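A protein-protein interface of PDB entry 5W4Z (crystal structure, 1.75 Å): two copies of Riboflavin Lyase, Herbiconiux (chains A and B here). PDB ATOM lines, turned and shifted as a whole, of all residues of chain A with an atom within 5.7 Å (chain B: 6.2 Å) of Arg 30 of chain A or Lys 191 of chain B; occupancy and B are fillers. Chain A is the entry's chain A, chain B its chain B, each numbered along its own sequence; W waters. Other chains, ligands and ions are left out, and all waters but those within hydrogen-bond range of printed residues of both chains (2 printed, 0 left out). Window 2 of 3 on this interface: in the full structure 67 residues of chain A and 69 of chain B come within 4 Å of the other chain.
NH1 of Arg 30 of chain A is in hydrogen-bond range of O of Lys 191 of chain B, 2.7 Å away.
NH1 of Arg 30 of chain A is in hydrogen-bond range of O of Gly 193 of chain B.
The side-chain amino group (NZ) of Lys 191 of chain B is in hydrogen-bond range of the backbone carbonyl oxygen (O) of His 31 of chain A (2.7 Å).
The backbone carbonyl oxygen of Pro 32 of chain A is in hydrogen-bond range of the side-chain amino group of Lys 191 of chain B (3.3 Å).
The side-chain amino group of Lys 191 of chain B lies within hydrogen-bond range of the backbone carbonyl oxygen of Asn 34 of chain A (2.7 Å).
The backbone carbonyl oxygen (O) of Val 81 of chain A lies within hydrogen-bond range of the backbone NH (N) of Tyr 195 of chain B (2.9 Å).
The backbone NH (N) of Trp 29 of chain A sits at hydrogen-bond distance from the side-chain amide oxygen (OD1) of Asn 22 of chain A, 3.1 Å away.
The backbone carbonyl oxygen of Thr 28 of chain A sits at hydrogen-bond distance from the side-chain amide nitrogen of Asn 34 of chain A (3.2 Å).
The backbone carbonyl oxygen of Arg 194 of chain B lies within hydrogen-bond range of the backbone NH of Arg 189 of chain B (3.3 Å).
The backbone carbonyl oxygen of Tyr 195 of chain B is in hydrogen-bond range of the backbone NH of Arg 189 of chain B (2.8 Å).
OD1 of Asp 190 of chain B is in hydrogen-bond range of N of Gln 192 of chain B, at 2.9 Å.
The side-chain carboxylate (OD1) of Asp 190 of chain B sits at hydrogen-bond distance from the backbone NH (N) of Gly 193 of chain B, 3.3 Å away.
Among the printed residues, merely in contact across the chains: Trp 29 of chain A with Arg 189 of chain B (3.9 Å), Trp 29 of chain A with Asp 190 of chain B (3.2 Å), Trp 29 of chain A with Lys 191 of chain B (3.3 Å), Trp 29 of chain A with Arg 194 of chain B (3.9 Å), Trp 29 of chain A with Tyr 195 of chain B (3.5 Å), Arg 30 of chain A with Asp 190 of chain B (3.7 Å), His 37 of chain A with Arg 189 of chain B (3.8 Å), His 37 of chain A with Lys 191 of chain B (3.8 Å) and Val 81 of chain A with Arg 194 of chain B (3.7 Å).
Asn 22 of chain A touches none of the printed residues of chain B.
Arg 30 of chain A touches three residues of chain B.
Printed residues of chain B within 4 Å of His 31 of chain A: Lys 191.
Of the printed residues of chain B, Pro 32 of chain A touches Lys 191 (3.3 Å).
Gln 35 of chain A touches none of the printed residues of chain B.
Of the printed residues of chain B, His 37 of chain A touches Arg 189 (3.8 Å) and Lys 191 (3.8 Å).
Of the printed residues of chain B, Val 81 of chain A touches Arg 194 and Tyr 195.
Of the printed residues of chain A, Arg 189 of chain B touches Trp 29 (3.9 Å) and His 37 (3.8 Å).
Lys 191 of chain B touches just these residues of chain A: Trp 29, Arg 30, His 31, Pro 32, Asn 34 and His 37.
The nearest residue of chain B that does not touch Arg 30 of chain A is Gln 192 of chain B (4.1 Å).
Of the 14 printed residues of chain A, 7 touch a printed residue of chain B.
No position is printed for both chains.
Water W1 lies within hydrogen-bond range of O of His 37 of chain A (2.8 Å), OH of Tyr 195 of chain B (2.8 Å) and NE of Arg 189 of chain B (3.0 Å).
Water W2 bridges the backbone carbonyl oxygen of His 37 of chain A and the guanidinium group of Arg 189 of chain B.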
ATOM      1  N   ASN A  22     -23.507  11.362  19.402  1.00  0.00           N
ATOM      2  CA  ASN A  22     -22.916  11.983  18.224  1.00  0.00           C
ATOM      3  C   ASN A  22     -24.001  12.181  17.173  1.00  0.00           C
ATOM      4  O   ASN A  22     -25.146  11.760  17.349  1.00  0.00           O
ATOM      5  CB  ASN A  22     -21.760  11.121  17.721  1.00  0.00           C
ATOM      6  CG  ASN A  22     -20.619  11.051  18.723  1.00  0.00           C
ATOM      7  OD1 ASN A  22     -20.077  12.080  19.121  1.00  0.00           O
ATOM      8  ND2 ASN A  22     -20.269   9.838  19.157  1.00  0.00           N
ATOM      9  N   ALA A  27     -18.154  12.071  15.062  1.00  0.00           N
ATOM     10  CA  ALA A  27     -18.064  11.696  16.474  1.00  0.00           C
ATOM     11  C   ALA A  27     -17.160  12.710  17.178  1.00  0.00           C
ATOM     12  O   ALA A  27     -15.957  12.489  17.317  1.00  0.00           O
ATOM     13  CB  ALA A  27     -17.546  10.275  16.638  1.00  0.00           C
ATOM     14  N   THR A  28     -17.760  13.809  17.638  1.00  0.00           N
ATOM     15  CA  THR A  28     -17.028  14.839  18.368  1.00  0.00           C
ATOM     16  C   THR A  28     -17.150  14.702  19.880  1.00  0.00           C
ATOM     17  O   THR A  28     -16.718  15.607  20.602  1.00  0.00           O
ATOM     18  CB  THR A  28     -17.510  16.231  17.958  1.00  0.00           C
ATOM     19  OG1 THR A  28     -18.927  16.323  18.174  1.00  0.00           O
ATOM     20  CG2 THR A  28     -17.190  16.501  16.495  1.00  0.00           C
ATOM     21  N   TRP A  29     -17.707  13.585  20.372  1.00  0.00           N
ATOM     22  CA  TRP A  29     -18.048  13.447  21.787  1.00  0.00           C
ATOM     23  C   TRP A  29     -16.848  13.586  22.718  1.00  0.00           C
ATOM     24  O   TRP A  29     -17.036  13.893  23.900  1.00  0.00           O
ATOM     25  CB  TRP A  29     -18.720  12.093  22.034  1.00  0.00           C
ATOM     26  CG  TRP A  29     -17.760  10.947  21.956  1.00  0.00           C
ATOM     27  CD1 TRP A  29     -17.193  10.421  20.825  1.00  0.00           C
ATOM     28  CD2 TRP A  29     -17.234  10.196  23.053  1.00  0.00           C
ATOM     29  NE1 TRP A  29     -16.351   9.385  21.153  1.00  0.00           N
ATOM     30  CE2 TRP A  29     -16.356   9.228  22.515  1.00  0.00           C
ATOM     31  CE3 TRP A  29     -17.413  10.250  24.438  1.00  0.00           C
ATOM     32  CZ2 TRP A  29     -15.669   8.315  23.315  1.00  0.00           C
ATOM     33  CZ3 TRP A  29     -16.724   9.346  25.233  1.00  0.00           C
ATOM     34  CH2 TRP A  29     -15.864   8.390  24.667  1.00  0.00           C
ATOM     35  N   ARG A  30     -15.627  13.361  22.229  1.00  0.00           N
ATOM     36  CA  ARG A  30     -14.449  13.397  23.092  1.00  0.00           C
ATOM     37  C   ARG A  30     -13.971  14.809  23.415  1.00  0.00           C
ATOM     38  O   ARG A  30     -13.125  14.962  24.305  1.00  0.00           O
ATOM     39  CB  ARG A  30     -13.292  12.627  22.452  1.00  0.00           C
ATOM     40  CG  ARG A  30     -13.526  11.142  22.304  1.00  0.00           C
ATOM     41  CD  ARG A  30     -12.247  10.442  21.878  1.00  0.00           C
ATOM     42  NE  ARG A  30     -12.486   9.038  21.578  1.00  0.00           N
ATOM     43  CZ  ARG A  30     -12.329   8.048  22.452  1.00  0.00           C
ATOM     44  NH1 ARG A  30     -11.920   8.300  23.693  1.00  0.00           N
ATOM     45  NH2 ARG A  30     -12.573   6.800  22.080  1.00  0.00           N
ATOM     46  N   HIS A  31     -14.456  15.822  22.702  1.00  0.00           N
ATOM     47  CA  HIS A  31     -14.069  17.194  22.998  1.00  0.00           C
ATOM     48  C   HIS A  31     -14.382  17.503  24.461  1.00  0.00           C
ATOM     49  O   HIS A  31     -15.444  17.111  24.963  1.00  0.00           O
ATOM     50  CB  HIS A  31     -14.809  18.166  22.075  1.00  0.00           C
ATOM     51  CG  HIS A  31     -14.347  19.586  22.188  1.00  0.00           C
ATOM     52  ND1 HIS A  31     -14.645  20.381  23.273  1.00  0.00           N
ATOM     53  CD2 HIS A  31     -13.615  20.356  21.346  1.00  0.00           C
ATOM     54  CE1 HIS A  31     -14.113  21.578  23.098  1.00  0.00           C
ATOM     55  NE2 HIS A  31     -13.486  21.590  21.935  1.00  0.00           N
ATOM     56  N   PRO A  32     -13.484  18.187  25.174  1.00  0.00           N
ATOM     57  CA  PRO A  32     -13.676  18.354  26.628  1.00  0.00           C
ATOM     58  C   PRO A  32     -14.938  19.109  27.012  1.00  0.00           C
ATOM     59  O   PRO A  32     -15.457  18.899  28.116  1.00  0.00           O
ATOM     60  CB  PRO A  32     -12.408  19.109  27.064  1.00  0.00           C
ATOM     61  CG  PRO A  32     -11.814  19.658  25.807  1.00  0.00           C
ATOM     62  CD  PRO A  32     -12.181  18.703  24.723  1.00  0.00           C
ATOM     63  N   ASP A  33     -15.462  19.971  26.141  1.00  0.00           N
ATOM     64  CA  ASP A  33     -16.641  20.770  26.450  1.00  0.00           C
ATOM     65  C   ASP A  33     -17.945  20.168  25.930  1.00  0.00           C
ATOM     66  O   ASP A  33     -19.019  20.714  26.208  1.00  0.00           O
ATOM     67  CB  ASP A  33     -16.465  22.182  25.890  1.00  0.00           C
ATOM     68  CG  ASP A  33     -15.195  22.850  26.396  1.00  0.00           C
ATOM     69  OD1 ASP A  33     -14.857  22.657  27.583  1.00  0.00           O
ATOM     70  OD2 ASP A  33     -14.531  23.555  25.605  1.00  0.00           O
ATOM     71  N   ASN A  34     -17.883  19.062  25.195  1.00  0.00           N
ATOM     72  CA  ASN A  34     -19.085  18.455  24.643  1.00  0.00           C
ATOM     73  C   ASN A  34     -19.833  17.694  25.736  1.00  0.00           C
ATOM     74  O   ASN A  34     -19.229  16.928  26.495  1.00  0.00           O
ATOM     75  CB  ASN A  34     -18.722  17.522  23.486  1.00  0.00           C
ATOM     76  CG  ASN A  34     -19.888  17.277  22.543  1.00  0.00           C
ATOM     77  OD1 ASN A  34     -21.039  17.540  22.881  1.00  0.00           O
ATOM     78  ND2 ASN A  34     -19.591  16.774  21.350  1.00  0.00           N
ATOM     79  N   GLN A  35     -21.150  17.903  25.811  1.00  0.00           N
ATOM     80  CA  GLN A  35     -21.974  17.310  26.858  1.00  0.00           C
ATOM     81  C   GLN A  35     -23.005  16.306  26.353  1.00  0.00           C
ATOM     82  O   GLN A  35     -23.786  15.794  27.164  1.00  0.00           O
ATOM     83  CB  GLN A  35     -22.705  18.411  27.645  1.00  0.00           C
ATOM     84  CG  GLN A  35     -21.797  19.516  28.188  1.00  0.00           C
ATOM     85  CD  GLN A  35     -20.836  19.013  29.234  1.00  0.00           C
ATOM     86  OE1 GLN A  35     -21.201  18.204  30.090  1.00  0.00           O
ATOM     87  NE2 GLN A  35     -19.592  19.487  29.174  1.00  0.00           N
ATOM     88  N   HIS A  37     -22.918  13.291  25.515  1.00  0.00           N
ATOM     89  CA  HIS A  37     -22.940  11.952  26.088  1.00  0.00           C
ATOM     90  C   HIS A  37     -23.986  11.825  27.186  1.00  0.00           C
ATOM     91  O   HIS A  37     -24.307  10.701  27.588  1.00  0.00           O
ATOM     92  CB  HIS A  37     -21.563  11.578  26.628  1.00  0.00           C
ATOM     93  CG  HIS A  37     -21.054  12.505  27.686  1.00  0.00           C
ATOM     94  ND1 HIS A  37     -20.558  13.760  27.400  1.00  0.00           N
ATOM     95  CD2 HIS A  37     -20.954  12.357  29.029  1.00  0.00           C
ATOM     96  CE1 HIS A  37     -20.180  14.347  28.521  1.00  0.00           C
ATOM     97  NE2 HIS A  37     -20.400  13.514  29.523  1.00  0.00           N
ATOM     98  N   VAL A  81     -16.773   1.874  20.473  1.00  0.00           N
ATOM     99  CA  VAL A  81     -15.675   2.621  21.084  1.00  0.00           C
ATOM    100  C   VAL A  81     -15.910   4.124  20.944  1.00  0.00           C
ATOM    101  O   VAL A  81     -15.578   4.907  21.843  1.00  0.00           O
ATOM    102  CB  VAL A  81     -14.330   2.187  20.467  1.00  0.00           C
ATOM    103  CG1 VAL A  81     -13.209   3.145  20.859  1.00  0.00           C
ATOM    104  CG2 VAL A  81     -13.982   0.769  20.897  1.00  0.00           C
ATOM    105  N   GLU A  82     -16.509   4.547  19.832  1.00  0.00           N
ATOM    106  CA  GLU A  82     -16.733   5.962  19.553  1.00  0.00           C
ATOM    107  C   GLU A  82     -18.184   6.402  19.707  1.00  0.00           C
ATOM    108  O   GLU A  82     -18.475   7.586  19.503  1.00  0.00           O
ATOM    109  CB  GLU A  82     -16.251   6.307  18.140  1.00  0.00           C
ATOM    110  CG  GLU A  82     -14.756   6.149  17.942  1.00  0.00           C
ATOM    111  CD  GLU A  82     -13.950   6.957  18.941  1.00  0.00           C
ATOM    112  OE1 GLU A  82     -14.318   8.121  19.208  1.00  0.00           O
ATOM    113  OE2 GLU A  82     -12.950   6.424  19.465  1.00  0.00           O
ATOM    114  N   SER A 307     -10.388  15.887  17.946  1.00  0.00           N
ATOM    115  CA  SER A 307     -11.035  14.840  18.726  1.00  0.00           C
ATOM    116  C   SER A 307     -11.701  13.774  17.863  1.00  0.00           C
ATOM    117  O   SER A 307     -12.223  12.796  18.406  1.00  0.00           O
ATOM    118  CB  SER A 307     -12.069  15.460  19.672  1.00  0.00           C
ATOM    119  OG  SER A 307     -13.109  16.089  18.942  1.00  0.00           O
ATOM    120  N   ARG B 189     -18.454   5.730  28.557  1.00  0.00           N
ATOM    121  CA  ARG B 189     -18.521   7.183  28.383  1.00  0.00           C
ATOM    122  C   ARG B 189     -17.228   7.866  28.825  1.00  0.00           C
ATOM    123  O   ARG B 189     -17.253   8.967  29.379  1.00  0.00           O
ATOM    124  CB  ARG B 189     -19.712   7.786  29.136  1.00  0.00           C
ATOM    125  CG  ARG B 189     -21.092   7.184  28.844  1.00  0.00           C
ATOM    126  CD  ARG B 189     -22.124   7.926  29.679  1.00  0.00           C
ATOM    127  NE  ARG B 189     -23.503   7.486  29.485  1.00  0.00           N
ATOM    128  CZ  ARG B 189     -24.145   6.663  30.309  1.00  0.00           C
ATOM    129  NH1 ARG B 189     -23.522   6.174  31.376  1.00  0.00           N
ATOM    130  NH2 ARG B 189     -25.409   6.326  30.070  1.00  0.00           N
ATOM    131  N   ASP B 190     -16.089   7.220  28.571  1.00  0.00           N
ATOM    132  CA  ASP B 190     -14.786   7.711  29.014  1.00  0.00           C
ATOM    133  C   ASP B 190     -14.110   8.435  27.851  1.00  0.00           C
ATOM    134  O   ASP B 190     -13.630   7.793  26.912  1.00  0.00           O
ATOM    135  CB  ASP B 190     -13.920   6.558  29.521  1.00  0.00           C
ATOM    136  CG  ASP B 190     -12.593   7.024  30.114  1.00  0.00           C
ATOM    137  OD1 ASP B 190     -12.198   8.192  29.911  1.00  0.00           O
ATOM    138  OD2 ASP B 190     -11.932   6.205  30.785  1.00  0.00           O
ATOM    139  N   LYS B 191     -14.043   9.769  27.931  1.00  0.00           N
ATOM    140  CA  LYS B 191     -13.477  10.550  26.832  1.00  0.00           C
ATOM    141  C   LYS B 191     -12.012  10.214  26.589  1.00  0.00           C
ATOM    142  O   LYS B 191     -11.534  10.341  25.456  1.00  0.00           O
ATOM    143  CB  LYS B 191     -13.634  12.047  27.101  1.00  0.00           C
ATOM    144  CG  LYS B 191     -15.080  12.526  27.067  1.00  0.00           C
ATOM    145  CD  LYS B 191     -15.166  14.051  27.041  1.00  0.00           C
ATOM    146  CE  LYS B 191     -16.621  14.510  27.112  1.00  0.00           C
ATOM    147  NZ  LYS B 191     -16.746  15.994  27.096  1.00  0.00           N
ATOM    148  N   GLN B 192     -11.288   9.794  27.629  1.00  0.00           N
ATOM    149  CA  GLN B 192      -9.908   9.337  27.500  1.00  0.00           C
ATOM    150  C   GLN B 192      -9.805   7.862  27.139  1.00  0.00           C
ATOM    151  O   GLN B 192      -8.691   7.359  26.965  1.00  0.00           O
ATOM    152  CB  GLN B 192      -9.129   9.583  28.801  1.00  0.00           C
ATOM    153  CG  GLN B 192      -9.338  10.946  29.425  1.00  0.00           C
ATOM    154  CD  GLN B 192      -9.072  12.074  28.457  1.00  0.00           C
ATOM    155  OE1 GLN B 192      -8.080  12.059  27.727  1.00  0.00           O
ATOM    156  NE2 GLN B 192      -9.964  13.059  28.437  1.00  0.00           N
ATOM    157  N   GLY B 193     -10.929   7.156  27.040  1.00  0.00           N
ATOM    158  CA  GLY B 193     -10.908   5.746  26.710  1.00  0.00           C
ATOM    159  C   GLY B 193     -11.993   5.340  25.734  1.00  0.00           C
ATOM    160  O   GLY B 193     -11.942   5.693  24.552  1.00  0.00           O
ATOM    161  N   ARG B 194     -12.988   4.607  26.226  1.00  0.00           N
ATOM    162  CA  ARG B 194     -14.040   4.022  25.408  1.00  0.00           C
ATOM    163  C   ARG B 194     -15.376   4.682  25.721  1.00  0.00           C
ATOM    164  O   ARG B 194     -15.656   5.004  26.880  1.00  0.00           O
ATOM    165  CB  ARG B 194     -14.142   2.516  25.674  1.00  0.00           C
ATOM    166  CG  ARG B 194     -13.867   1.625  24.486  1.00  0.00           C
ATOM    167  CD  ARG B 194     -13.295   0.278  24.924  1.00  0.00           C
ATOM    168  NE  ARG B 194     -13.823  -0.184  26.209  1.00  0.00           N
ATOM    169  CZ  ARG B 194     -13.651  -1.416  26.688  1.00  0.00           C
ATOM    170  NH1 ARG B 194     -12.980  -2.316  25.984  1.00  0.00           N
ATOM    171  NH2 ARG B 194     -14.153  -1.755  27.869  1.00  0.00           N
ATOM    172  N   TYR B 195     -16.201   4.887  24.685  1.00  0.00           N
ATOM    173  CA  TYR B 195     -17.597   5.234  24.937  1.00  0.00           C
ATOM    174  C   TYR B 195     -18.369   4.018  25.430  1.00  0.00           C
ATOM    175  O   TYR B 195     -19.162   4.112  26.377  1.00  0.00           O
ATOM    176  CB  TYR B 195     -18.257   5.810  23.675  1.00  0.00           C
ATOM    177  CG  TYR B 195     -19.734   6.088  23.866  1.00  0.00           C
ATOM    178  CD1 TYR B 195     -20.165   7.275  24.439  1.00  0.00           C
ATOM    179  CD2 TYR B 195     -20.696   5.152  23.504  1.00  0.00           C
ATOM    180  CE1 TYR B 195     -21.505   7.532  24.637  1.00  0.00           C
ATOM    181  CE2 TYR B 195     -22.049   5.399  23.701  1.00  0.00           C
ATOM    182  CZ  TYR B 195     -22.445   6.591  24.264  1.00  0.00           C
ATOM    183  OH  TYR B 195     -23.784   6.844  24.462  1.00  0.00           O
HETATM  184  O   HOH W   1     -24.782   8.048  26.796  1.00  0.00           O
HETATM  185  O   HOH W   2     -25.242   9.743  30.177  1.00  0.00           O
